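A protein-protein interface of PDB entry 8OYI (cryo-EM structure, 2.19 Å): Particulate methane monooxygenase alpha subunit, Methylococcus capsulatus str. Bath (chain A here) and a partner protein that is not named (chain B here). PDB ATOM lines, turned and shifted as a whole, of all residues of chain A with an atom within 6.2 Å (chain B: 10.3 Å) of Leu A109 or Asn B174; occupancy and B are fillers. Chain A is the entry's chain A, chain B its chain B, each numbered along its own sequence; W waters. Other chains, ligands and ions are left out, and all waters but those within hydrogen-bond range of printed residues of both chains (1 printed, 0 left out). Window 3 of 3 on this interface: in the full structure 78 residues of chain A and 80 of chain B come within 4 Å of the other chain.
Hydrophobic or aromatic side chains of chain B within 4 Å of the printed part of chain A: Tyr B173, Met B176, Met B178 and Tyr B186. Along chain B the printed residues that touch a printed residue of chain A span positions 173 to 186. Printed residues of chain A that touch a printed residue of chain B: Lys A101, Glu A102, Ser A103, Leu A109, Pro A111 and Arg A112. Hydrophobic or aromatic side chains of chain A within 4 Å of the printed part of chain B: Leu A109 and Pro A111. Among the printed residues, no Asp or Glu carboxylate lies within 4 Å of a Lys or Arg side-chain nitrogen of the other chain.
The side-chain carboxylate (OE1) of Glu A102 lies within hydrogen-bond range of the side-chain hydroxyl (OH) of Tyr A104, at 3.2 Å. The backbone carbonyl oxygen (O) of Ser A103 sits at hydrogen-bond distance from the backbone NH (N) of Val A110. N of Val B171 sits at hydrogen-bond distance from O of Met B178 (2.8 Å). The side-chain carboxylate (OE2) of Glu B172 sits at hydrogen-bond distance from the backbone NH (N) of Met B176 (3.3 Å). OH of Tyr B173 is in hydrogen-bond range of ND2 of Asn B187, 3.2 Å away.
Water W1 bridges O of Leu B177 and NH2 of Arg A112.
O of Lys A101 sits at hydrogen-bond distance from OH of Tyr B173 (2.7 Å). The side-chain hydroxyl (OH) of Tyr B186 is in hydrogen-bond range of the backbone NH (N) of Ser A103 (2.6 Å).
OD1 of Asn B174 touches O of Lys A101 (3.99 Å). CE2 of Tyr B186 touches O of Lys A101, 3.4 Å away. CG of Glu A102 touches OD1 of Asn B174, 3.5 Å away. Glu A102 touches Tyr B186. Tyr B173 touches Leu A109 (O to CD2, 3.98 Å). Asn B174 touches Leu A109 (CB to CD1, 3.9 Å). Tyr B186 touches Leu A109. Pro A111 touches Met B178. Tyr B186 touches Pro A111 (CE1 to CA, 3.5 Å). Met B176 touches Arg A112 (CE to NH2, 3.3 Å).
Of the printed residues of chain B, Leu A109 touches Tyr B173, Asn B174 and Tyr B186. Of the printed residues of chain A, Asn B174 touches Lys A101 (3.99 Å), Glu A102 (3.5 Å) and Leu A109 (3.9 Å). Glu A102 touches two residues of chain B. Of chain B, only Tyr B186 comes within 4 Å of Ser A103. No residue of chain B comes within 4 Å of Gly A107. No residue of chain B comes within 4 Å of Gln A108. No residue of chain B comes within 4 Å of Val A110. Of the printed residues of chain B, Lys A101 touches Tyr B173, Asn B174 and Tyr B186. Printed residues of chain A within 4 Å of Met B178: Pro A111 (3.8 Å). Of the printed residues of chain B, Arg A112 touches Met B176 (3.3 Å). Of the printed residues of chain B, Pro A111 touches Met B176 (3.6 Å), Met B178 (3.8 Å) and Tyr B186 (3.5 Å). Printed residues of chain A within 4 Å of Met B176: Pro A111 (3.6 Å) and Arg A112 (3.3 Å). Asn B187 touches none of the printed residues of chain A. Tyr A104 touches none of the printed residues of chain B. The nearest printed residue of chain B that does not touch Leu A109 is Met B176 (4.2 Å).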
ATOM      1  N   LYS A 101     -25.321 -10.478 -28.766  1.00  0.00           N
ATOM      2  CA  LYS A 101     -24.036  -9.807 -28.602  1.00  0.00           C
ATOM      3  C   LYS A 101     -23.100 -10.634 -27.730  1.00  0.00           C
ATOM      4  O   LYS A 101     -21.932 -10.845 -28.073  1.00  0.00           O
ATOM      5  CB  LYS A 101     -24.246  -8.414 -28.003  1.00  0.00           C
ATOM      6  CG  LYS A 101     -24.490  -7.326 -29.035  1.00  0.00           C
ATOM      7  CD  LYS A 101     -23.462  -7.372 -30.153  1.00  0.00           C
ATOM      8  CE  LYS A 101     -22.085  -6.965 -29.660  1.00  0.00           C
ATOM      9  NZ  LYS A 101     -21.137  -6.719 -30.781  1.00  0.00           N
ATOM     10  N   GLU A 102     -23.605 -11.126 -26.601  1.00  0.00           N
ATOM     11  CA  GLU A 102     -22.803 -11.910 -25.677  1.00  0.00           C
ATOM     12  C   GLU A 102     -23.689 -12.947 -25.003  1.00  0.00           C
ATOM     13  O   GLU A 102     -24.905 -12.779 -24.893  1.00  0.00           O
ATOM     14  CB  GLU A 102     -22.132 -11.034 -24.615  1.00  0.00           C
ATOM     15  CG  GLU A 102     -21.023 -10.134 -25.127  1.00  0.00           C
ATOM     16  CD  GLU A 102     -21.164  -8.708 -24.641  1.00  0.00           C
ATOM     17  OE1 GLU A 102     -21.386  -8.512 -23.429  1.00  0.00           O
ATOM     18  OE2 GLU A 102     -21.052  -7.782 -25.471  1.00  0.00           O
ATOM     19  N   SER A 103     -23.056 -14.022 -24.545  1.00  0.00           N
ATOM     20  CA  SER A 103     -23.726 -15.041 -23.748  1.00  0.00           C
ATOM     21  C   SER A 103     -22.702 -15.624 -22.786  1.00  0.00           C
ATOM     22  O   SER A 103     -21.562 -15.885 -23.178  1.00  0.00           O
ATOM     23  CB  SER A 103     -24.330 -16.143 -24.625  1.00  0.00           C
ATOM     24  OG  SER A 103     -23.374 -16.651 -25.537  1.00  0.00           O
ATOM     25  N   TYR A 104     -23.106 -15.818 -21.534  1.00  0.00           N
ATOM     26  CA  TYR A 104     -22.203 -16.285 -20.496  1.00  0.00           C
ATOM     27  C   TYR A 104     -22.830 -17.439 -19.732  1.00  0.00           C
ATOM     28  O   TYR A 104     -24.035 -17.440 -19.468  1.00  0.00           O
ATOM     29  CB  TYR A 104     -21.845 -15.161 -19.512  1.00  0.00           C
ATOM     30  CG  TYR A 104     -21.225 -13.946 -20.153  1.00  0.00           C
ATOM     31  CD1 TYR A 104     -22.016 -12.941 -20.692  1.00  0.00           C
ATOM     32  CD2 TYR A 104     -19.848 -13.800 -20.223  1.00  0.00           C
ATOM     33  CE1 TYR A 104     -21.456 -11.829 -21.277  1.00  0.00           C
ATOM     34  CE2 TYR A 104     -19.276 -12.689 -20.809  1.00  0.00           C
ATOM     35  CZ  TYR A 104     -20.084 -11.708 -21.335  1.00  0.00           C
ATOM     36  OH  TYR A 104     -19.522 -10.600 -21.920  1.00  0.00           O
ATOM     37  N   ILE A 105     -22.007 -18.424 -19.392  1.00  0.00           N
ATOM     38  CA  ILE A 105     -22.355 -19.450 -18.418  1.00  0.00           C
ATOM     39  C   ILE A 105     -21.325 -19.360 -17.302  1.00  0.00           C
ATOM     40  O   ILE A 105     -20.122 -19.520 -17.545  1.00  0.00           O
ATOM     41  CB  ILE A 105     -22.382 -20.855 -19.043  1.00  0.00           C
ATOM     42  CG1 ILE A 105     -23.477 -20.937 -20.110  1.00  0.00           C
ATOM     43  CG2 ILE A 105     -22.582 -21.911 -17.963  1.00  0.00           C
ATOM     44  CD1 ILE A 105     -23.891 -22.349 -20.460  1.00  0.00           C
ATOM     45  N   GLY A 107     -19.372 -16.965 -15.571  1.00  0.00           N
ATOM     46  CA  GLY A 107     -19.008 -15.580 -15.787  1.00  0.00           C
ATOM     47  C   GLY A 107     -18.204 -15.393 -17.059  1.00  0.00           C
ATOM     48  O   GLY A 107     -17.676 -14.309 -17.317  1.00  0.00           O
ATOM     49  N   GLN A 108     -18.113 -16.448 -17.860  1.00  0.00           N
ATOM     50  CA  GLN A 108     -17.250 -16.484 -19.030  1.00  0.00           C
ATOM     51  C   GLN A 108     -18.065 -16.651 -20.306  1.00  0.00           C
ATOM     52  O   GLN A 108     -19.096 -17.330 -20.313  1.00  0.00           O
ATOM     53  CB  GLN A 108     -16.221 -17.605 -18.893  1.00  0.00           C
ATOM     54  CG  GLN A 108     -16.820 -18.990 -18.830  1.00  0.00           C
ATOM     55  CD  GLN A 108     -16.008 -20.004 -19.596  1.00  0.00           C
ATOM     56  OE1 GLN A 108     -16.085 -20.071 -20.820  1.00  0.00           O
ATOM     57  NE2 GLN A 108     -15.224 -20.801 -18.882  1.00  0.00           N
ATOM     58  N   LEU A 109     -17.594 -16.021 -21.381  1.00  0.00           N
ATOM     59  CA  LEU A 109     -18.321 -16.021 -22.642  1.00  0.00           C
ATOM     60  C   LEU A 109     -18.357 -17.415 -23.253  1.00  0.00           C
ATOM     61  O   LEU A 109     -17.375 -18.158 -23.205  1.00  0.00           O
ATOM     62  CB  LEU A 109     -17.672 -15.031 -23.613  1.00  0.00           C
ATOM     63  CG  LEU A 109     -18.440 -14.706 -24.894  1.00  0.00           C
ATOM     64  CD1 LEU A 109     -19.237 -13.425 -24.723  1.00  0.00           C
ATOM     65  CD2 LEU A 109     -17.488 -14.596 -26.068  1.00  0.00           C
ATOM     66  N   VAL A 110     -19.498 -17.766 -23.837  1.00  0.00           N
ATOM     67  CA  VAL A 110     -19.699 -19.109 -24.375  1.00  0.00           C
ATOM     68  C   VAL A 110     -20.207 -19.034 -25.811  1.00  0.00           C
ATOM     69  O   VAL A 110     -21.363 -19.385 -26.082  1.00  0.00           O
ATOM     70  CB  VAL A 110     -20.653 -19.919 -23.483  1.00  0.00           C
ATOM     71  CG1 VAL A 110     -19.931 -20.361 -22.226  1.00  0.00           C
ATOM     72  CG2 VAL A 110     -21.874 -19.094 -23.106  1.00  0.00           C
ATOM     73  N   PRO A 111     -19.383 -18.602 -26.772  1.00  0.00           N
ATOM     74  CA  PRO A 111     -19.836 -18.586 -28.169  1.00  0.00           C
ATOM     75  C   PRO A 111     -19.903 -19.964 -28.801  1.00  0.00           C
ATOM     76  O   PRO A 111     -20.449 -20.091 -29.905  1.00  0.00           O
ATOM     77  CB  PRO A 111     -18.789 -17.711 -28.865  1.00  0.00           C
ATOM     78  CG  PRO A 111     -17.552 -17.943 -28.077  1.00  0.00           C
ATOM     79  CD  PRO A 111     -17.982 -18.162 -26.646  1.00  0.00           C
ATOM     80  N   ARG A 112     -19.367 -20.987 -28.150  1.00  0.00           N
ATOM     81  CA  ARG A 112     -19.366 -22.350 -28.651  1.00  0.00           C
ATOM     82  C   ARG A 112     -20.194 -23.236 -27.727  1.00  0.00           C
ATOM     83  O   ARG A 112     -20.723 -22.792 -26.705  1.00  0.00           O
ATOM     84  CB  ARG A 112     -17.935 -22.871 -28.778  1.00  0.00           C
ATOM     85  CG  ARG A 112     -16.948 -21.849 -29.316  1.00  0.00           C
ATOM     86  CD  ARG A 112     -15.791 -22.525 -30.019  1.00  0.00           C
ATOM     87  NE  ARG A 112     -14.525 -21.834 -29.801  1.00  0.00           N
ATOM     88  CZ  ARG A 112     -13.455 -22.396 -29.259  1.00  0.00           C
ATOM     89  NH1 ARG A 112     -13.466 -23.650 -28.846  1.00  0.00           N
ATOM     90  NH2 ARG A 112     -12.341 -21.680 -29.134  1.00  0.00           N
ATOM     91  N   MET A 269     -16.522 -26.377 -25.222  1.00  0.00           N
ATOM     92  CA  MET A 269     -15.722 -25.761 -24.175  1.00  0.00           C
ATOM     93  C   MET A 269     -16.037 -26.436 -22.846  1.00  0.00           C
ATOM     94  O   MET A 269     -17.194 -26.459 -22.414  1.00  0.00           O
ATOM     95  CB  MET A 269     -15.999 -24.262 -24.104  1.00  0.00           C
ATOM     96  CG  MET A 269     -15.366 -23.478 -25.244  1.00  0.00           C
ATOM     97  SD  MET A 269     -15.952 -21.778 -25.335  1.00  0.00           S
ATOM     98  CE  MET A 269     -15.636 -21.236 -23.664  1.00  0.00           C
ATOM     99  N   MET A 272     -16.989 -25.441 -17.381  1.00  0.00           N
ATOM    100  CA  MET A 272     -17.991 -24.455 -16.992  1.00  0.00           C
ATOM    101  C   MET A 272     -18.064 -24.426 -15.473  1.00  0.00           C
ATOM    102  O   MET A 272     -18.158 -25.475 -14.830  1.00  0.00           O
ATOM    103  CB  MET A 272     -19.349 -24.788 -17.603  1.00  0.00           C
ATOM    104  CG  MET A 272     -19.385 -24.810 -19.126  1.00  0.00           C
ATOM    105  SD  MET A 272     -19.095 -23.199 -19.888  1.00  0.00           S
ATOM    106  CE  MET A 272     -17.340 -23.271 -20.241  1.00  0.00           C
ATOM    107  N   VAL B 171     -10.860 -11.723 -35.415  1.00  0.00           N
ATOM    108  CA  VAL B 171     -11.430 -10.664 -34.593  1.00  0.00           C
ATOM    109  C   VAL B 171     -11.288 -11.055 -33.130  1.00  0.00           C
ATOM    110  O   VAL B 171     -11.529 -12.206 -32.758  1.00  0.00           O
ATOM    111  CB  VAL B 171     -12.908 -10.395 -34.938  1.00  0.00           C
ATOM    112  CG1 VAL B 171     -13.479  -9.335 -34.017  1.00  0.00           C
ATOM    113  CG2 VAL B 171     -13.057  -9.975 -36.392  1.00  0.00           C
ATOM    114  N   GLU B 172     -10.897 -10.092 -32.303  1.00  0.00           N
ATOM    115  CA  GLU B 172     -10.840 -10.277 -30.856  1.00  0.00           C
ATOM    116  C   GLU B 172     -12.215  -9.929 -30.302  1.00  0.00           C
ATOM    117  O   GLU B 172     -12.551  -8.755 -30.134  1.00  0.00           O
ATOM    118  CB  GLU B 172      -9.748  -9.398 -30.255  1.00  0.00           C
ATOM    119  CG  GLU B 172      -9.178  -9.897 -28.949  1.00  0.00           C
ATOM    120  CD  GLU B 172     -10.207  -9.985 -27.857  1.00  0.00           C
ATOM    121  OE1 GLU B 172     -10.790  -8.942 -27.489  1.00  0.00           O
ATOM    122  OE2 GLU B 172     -10.443 -11.109 -27.375  1.00  0.00           O
ATOM    123  N   TYR B 173     -13.023 -10.947 -30.017  1.00  0.00           N
ATOM    124  CA  TYR B 173     -14.431 -10.761 -29.663  1.00  0.00           C
ATOM    125  C   TYR B 173     -14.646 -11.164 -28.208  1.00  0.00           C
ATOM    126  O   TYR B 173     -14.751 -12.355 -27.900  1.00  0.00           O
ATOM    127  CB  TYR B 173     -15.332 -11.565 -30.598  1.00  0.00           C
ATOM    128  CG  TYR B 173     -16.787 -11.158 -30.550  1.00  0.00           C
ATOM    129  CD1 TYR B 173     -17.242 -10.050 -31.249  1.00  0.00           C
ATOM    130  CD2 TYR B 173     -17.705 -11.888 -29.809  1.00  0.00           C
ATOM    131  CE1 TYR B 173     -18.569  -9.678 -31.210  1.00  0.00           C
ATOM    132  CE2 TYR B 173     -19.038 -11.523 -29.764  1.00  0.00           C
ATOM    133  CZ  TYR B 173     -19.461 -10.419 -30.467  1.00  0.00           C
ATOM    134  OH  TYR B 173     -20.787 -10.050 -30.423  1.00  0.00           O
ATOM    135  N   ASN B 174     -14.720 -10.163 -27.329  1.00  0.00           N
ATOM    136  CA  ASN B 174     -15.053 -10.362 -25.914  1.00  0.00           C
ATOM    137  C   ASN B 174     -14.136 -11.387 -25.253  1.00  0.00           C
ATOM    138  O   ASN B 174     -14.583 -12.271 -24.519  1.00  0.00           O
ATOM    139  CB  ASN B 174     -16.521 -10.759 -25.750  1.00  0.00           C
ATOM    140  CG  ASN B 174     -17.471  -9.655 -26.170  1.00  0.00           C
ATOM    141  OD1 ASN B 174     -18.201  -9.790 -27.152  1.00  0.00           O
ATOM    142  ND2 ASN B 174     -17.471  -8.560 -25.425  1.00  0.00           N
ATOM    143  N   GLY B 175     -12.836 -11.267 -25.510  1.00  0.00           N
ATOM    144  CA  GLY B 175     -11.849 -12.121 -24.886  1.00  0.00           C
ATOM    145  C   GLY B 175     -11.518 -13.392 -25.639  1.00  0.00           C
ATOM    146  O   GLY B 175     -10.544 -14.065 -25.284  1.00  0.00           O
ATOM    147  N   MET B 176     -12.284 -13.738 -26.669  1.00  0.00           N
ATOM    148  CA  MET B 176     -12.076 -14.961 -27.428  1.00  0.00           C
ATOM    149  C   MET B 176     -11.775 -14.624 -28.882  1.00  0.00           C
ATOM    150  O   MET B 176     -12.304 -13.652 -29.426  1.00  0.00           O
ATOM    151  CB  MET B 176     -13.302 -15.872 -27.341  1.00  0.00           C
ATOM    152  CG  MET B 176     -13.377 -16.680 -26.053  1.00  0.00           C
ATOM    153  SD  MET B 176     -14.427 -18.140 -26.179  1.00  0.00           S
ATOM    154  CE  MET B 176     -13.473 -19.152 -27.303  1.00  0.00           C
ATOM    155  N   LEU B 177     -10.918 -15.429 -29.505  1.00  0.00           N
ATOM    156  CA  LEU B 177     -10.606 -15.250 -30.916  1.00  0.00           C
ATOM    157  C   LEU B 177     -11.726 -15.848 -31.757  1.00  0.00           C
ATOM    158  O   LEU B 177     -12.113 -17.004 -31.553  1.00  0.00           O
ATOM    159  CB  LEU B 177      -9.270 -15.894 -31.269  1.00  0.00           C
ATOM    160  CG  LEU B 177      -8.910 -15.776 -32.753  1.00  0.00           C
ATOM    161  CD1 LEU B 177      -8.547 -14.345 -33.095  1.00  0.00           C
ATOM    162  CD2 LEU B 177      -7.786 -16.715 -33.139  1.00  0.00           C
ATOM    163  N   MET B 178     -12.243 -15.065 -32.696  1.00  0.00           N
ATOM    164  CA  MET B 178     -13.314 -15.513 -33.573  1.00  0.00           C
ATOM    165  C   MET B 178     -13.106 -14.922 -34.958  1.00  0.00           C
ATOM    166  O   MET B 178     -12.653 -13.785 -35.102  1.00  0.00           O
ATOM    167  CB  MET B 178     -14.691 -15.106 -33.034  1.00  0.00           C
ATOM    168  CG  MET B 178     -15.199 -15.964 -31.890  1.00  0.00           C
ATOM    169  SD  MET B 178     -16.686 -15.293 -31.125  1.00  0.00           S
ATOM    170  CE  MET B 178     -17.955 -16.006 -32.167  1.00  0.00           C
ATOM    171  N   ASP B 182     -17.589 -16.670 -37.756  1.00  0.00           N
ATOM    172  CA  ASP B 182     -17.944 -17.128 -36.419  1.00  0.00           C
ATOM    173  C   ASP B 182     -18.825 -16.108 -35.711  1.00  0.00           C
ATOM    174  O   ASP B 182     -19.824 -16.469 -35.077  1.00  0.00           O
ATOM    175  CB  ASP B 182     -16.685 -17.398 -35.597  1.00  0.00           C
ATOM    176  CG  ASP B 182     -15.988 -18.683 -35.998  1.00  0.00           C
ATOM    177  OD1 ASP B 182     -16.653 -19.739 -36.027  1.00  0.00           O
ATOM    178  OD2 ASP B 182     -14.775 -18.631 -36.286  1.00  0.00           O
ATOM    179  N   ILE B 183     -18.475 -14.825 -35.816  1.00  0.00           N
ATOM    180  CA  ILE B 183     -19.273 -13.781 -35.179  1.00  0.00           C
ATOM    181  C   ILE B 183     -20.642 -13.678 -35.838  1.00  0.00           C
ATOM    182  O   ILE B 183     -21.643 -13.408 -35.168  1.00  0.00           O
ATOM    183  CB  ILE B 183     -18.522 -12.439 -35.214  1.00  0.00           C
ATOM    184  CG1 ILE B 183     -17.246 -12.537 -34.386  1.00  0.00           C
ATOM    185  CG2 ILE B 183     -19.390 -11.319 -34.666  1.00  0.00           C
ATOM    186  CD1 ILE B 183     -16.298 -11.417 -34.637  1.00  0.00           C
ATOM    187  N   TYR B 186     -22.650 -16.440 -34.415  1.00  0.00           N
ATOM    188  CA  TYR B 186     -22.959 -16.142 -33.022  1.00  0.00           C
ATOM    189  C   TYR B 186     -24.067 -15.104 -32.898  1.00  0.00           C
ATOM    190  O   TYR B 186     -25.025 -15.295 -32.141  1.00  0.00           O
ATOM    191  CB  TYR B 186     -21.694 -15.665 -32.313  1.00  0.00           C
ATOM    192  CG  TYR B 186     -21.831 -15.505 -30.822  1.00  0.00           C
ATOM    193  CD1 TYR B 186     -22.345 -16.526 -30.037  1.00  0.00           C
ATOM    194  CD2 TYR B 186     -21.432 -14.334 -30.195  1.00  0.00           C
ATOM    195  CE1 TYR B 186     -22.468 -16.380 -28.673  1.00  0.00           C
ATOM    196  CE2 TYR B 186     -21.549 -14.181 -28.832  1.00  0.00           C
ATOM    197  CZ  TYR B 186     -22.067 -15.207 -28.075  1.00  0.00           C
ATOM    198  OH  TYR B 186     -22.179 -15.051 -26.717  1.00  0.00           O
ATOM    199  N   ASN B 187     -23.953 -14.001 -33.633  1.00  0.00           N
ATOM    200  CA  ASN B 187     -24.870 -12.874 -33.520  1.00  0.00           C
ATOM    201  C   ASN B 187     -26.242 -13.208 -34.087  1.00  0.00           C
ATOM    202  O   ASN B 187     -27.258 -13.038 -33.409  1.00  0.00           O
ATOM    203  CB  ASN B 187     -24.301 -11.649 -34.241  1.00  0.00           C
ATOM    204  CG  ASN B 187     -23.141 -11.021 -33.499  1.00  0.00           C
ATOM    205  OD1 ASN B 187     -22.474 -10.128 -34.017  1.00  0.00           O
ATOM    206  ND2 ASN B 187     -22.894 -11.481 -32.280  1.00  0.00           N
HETATM  207  O   HOH W   1     -11.162 -19.432 -30.449  1.00  0.00           O
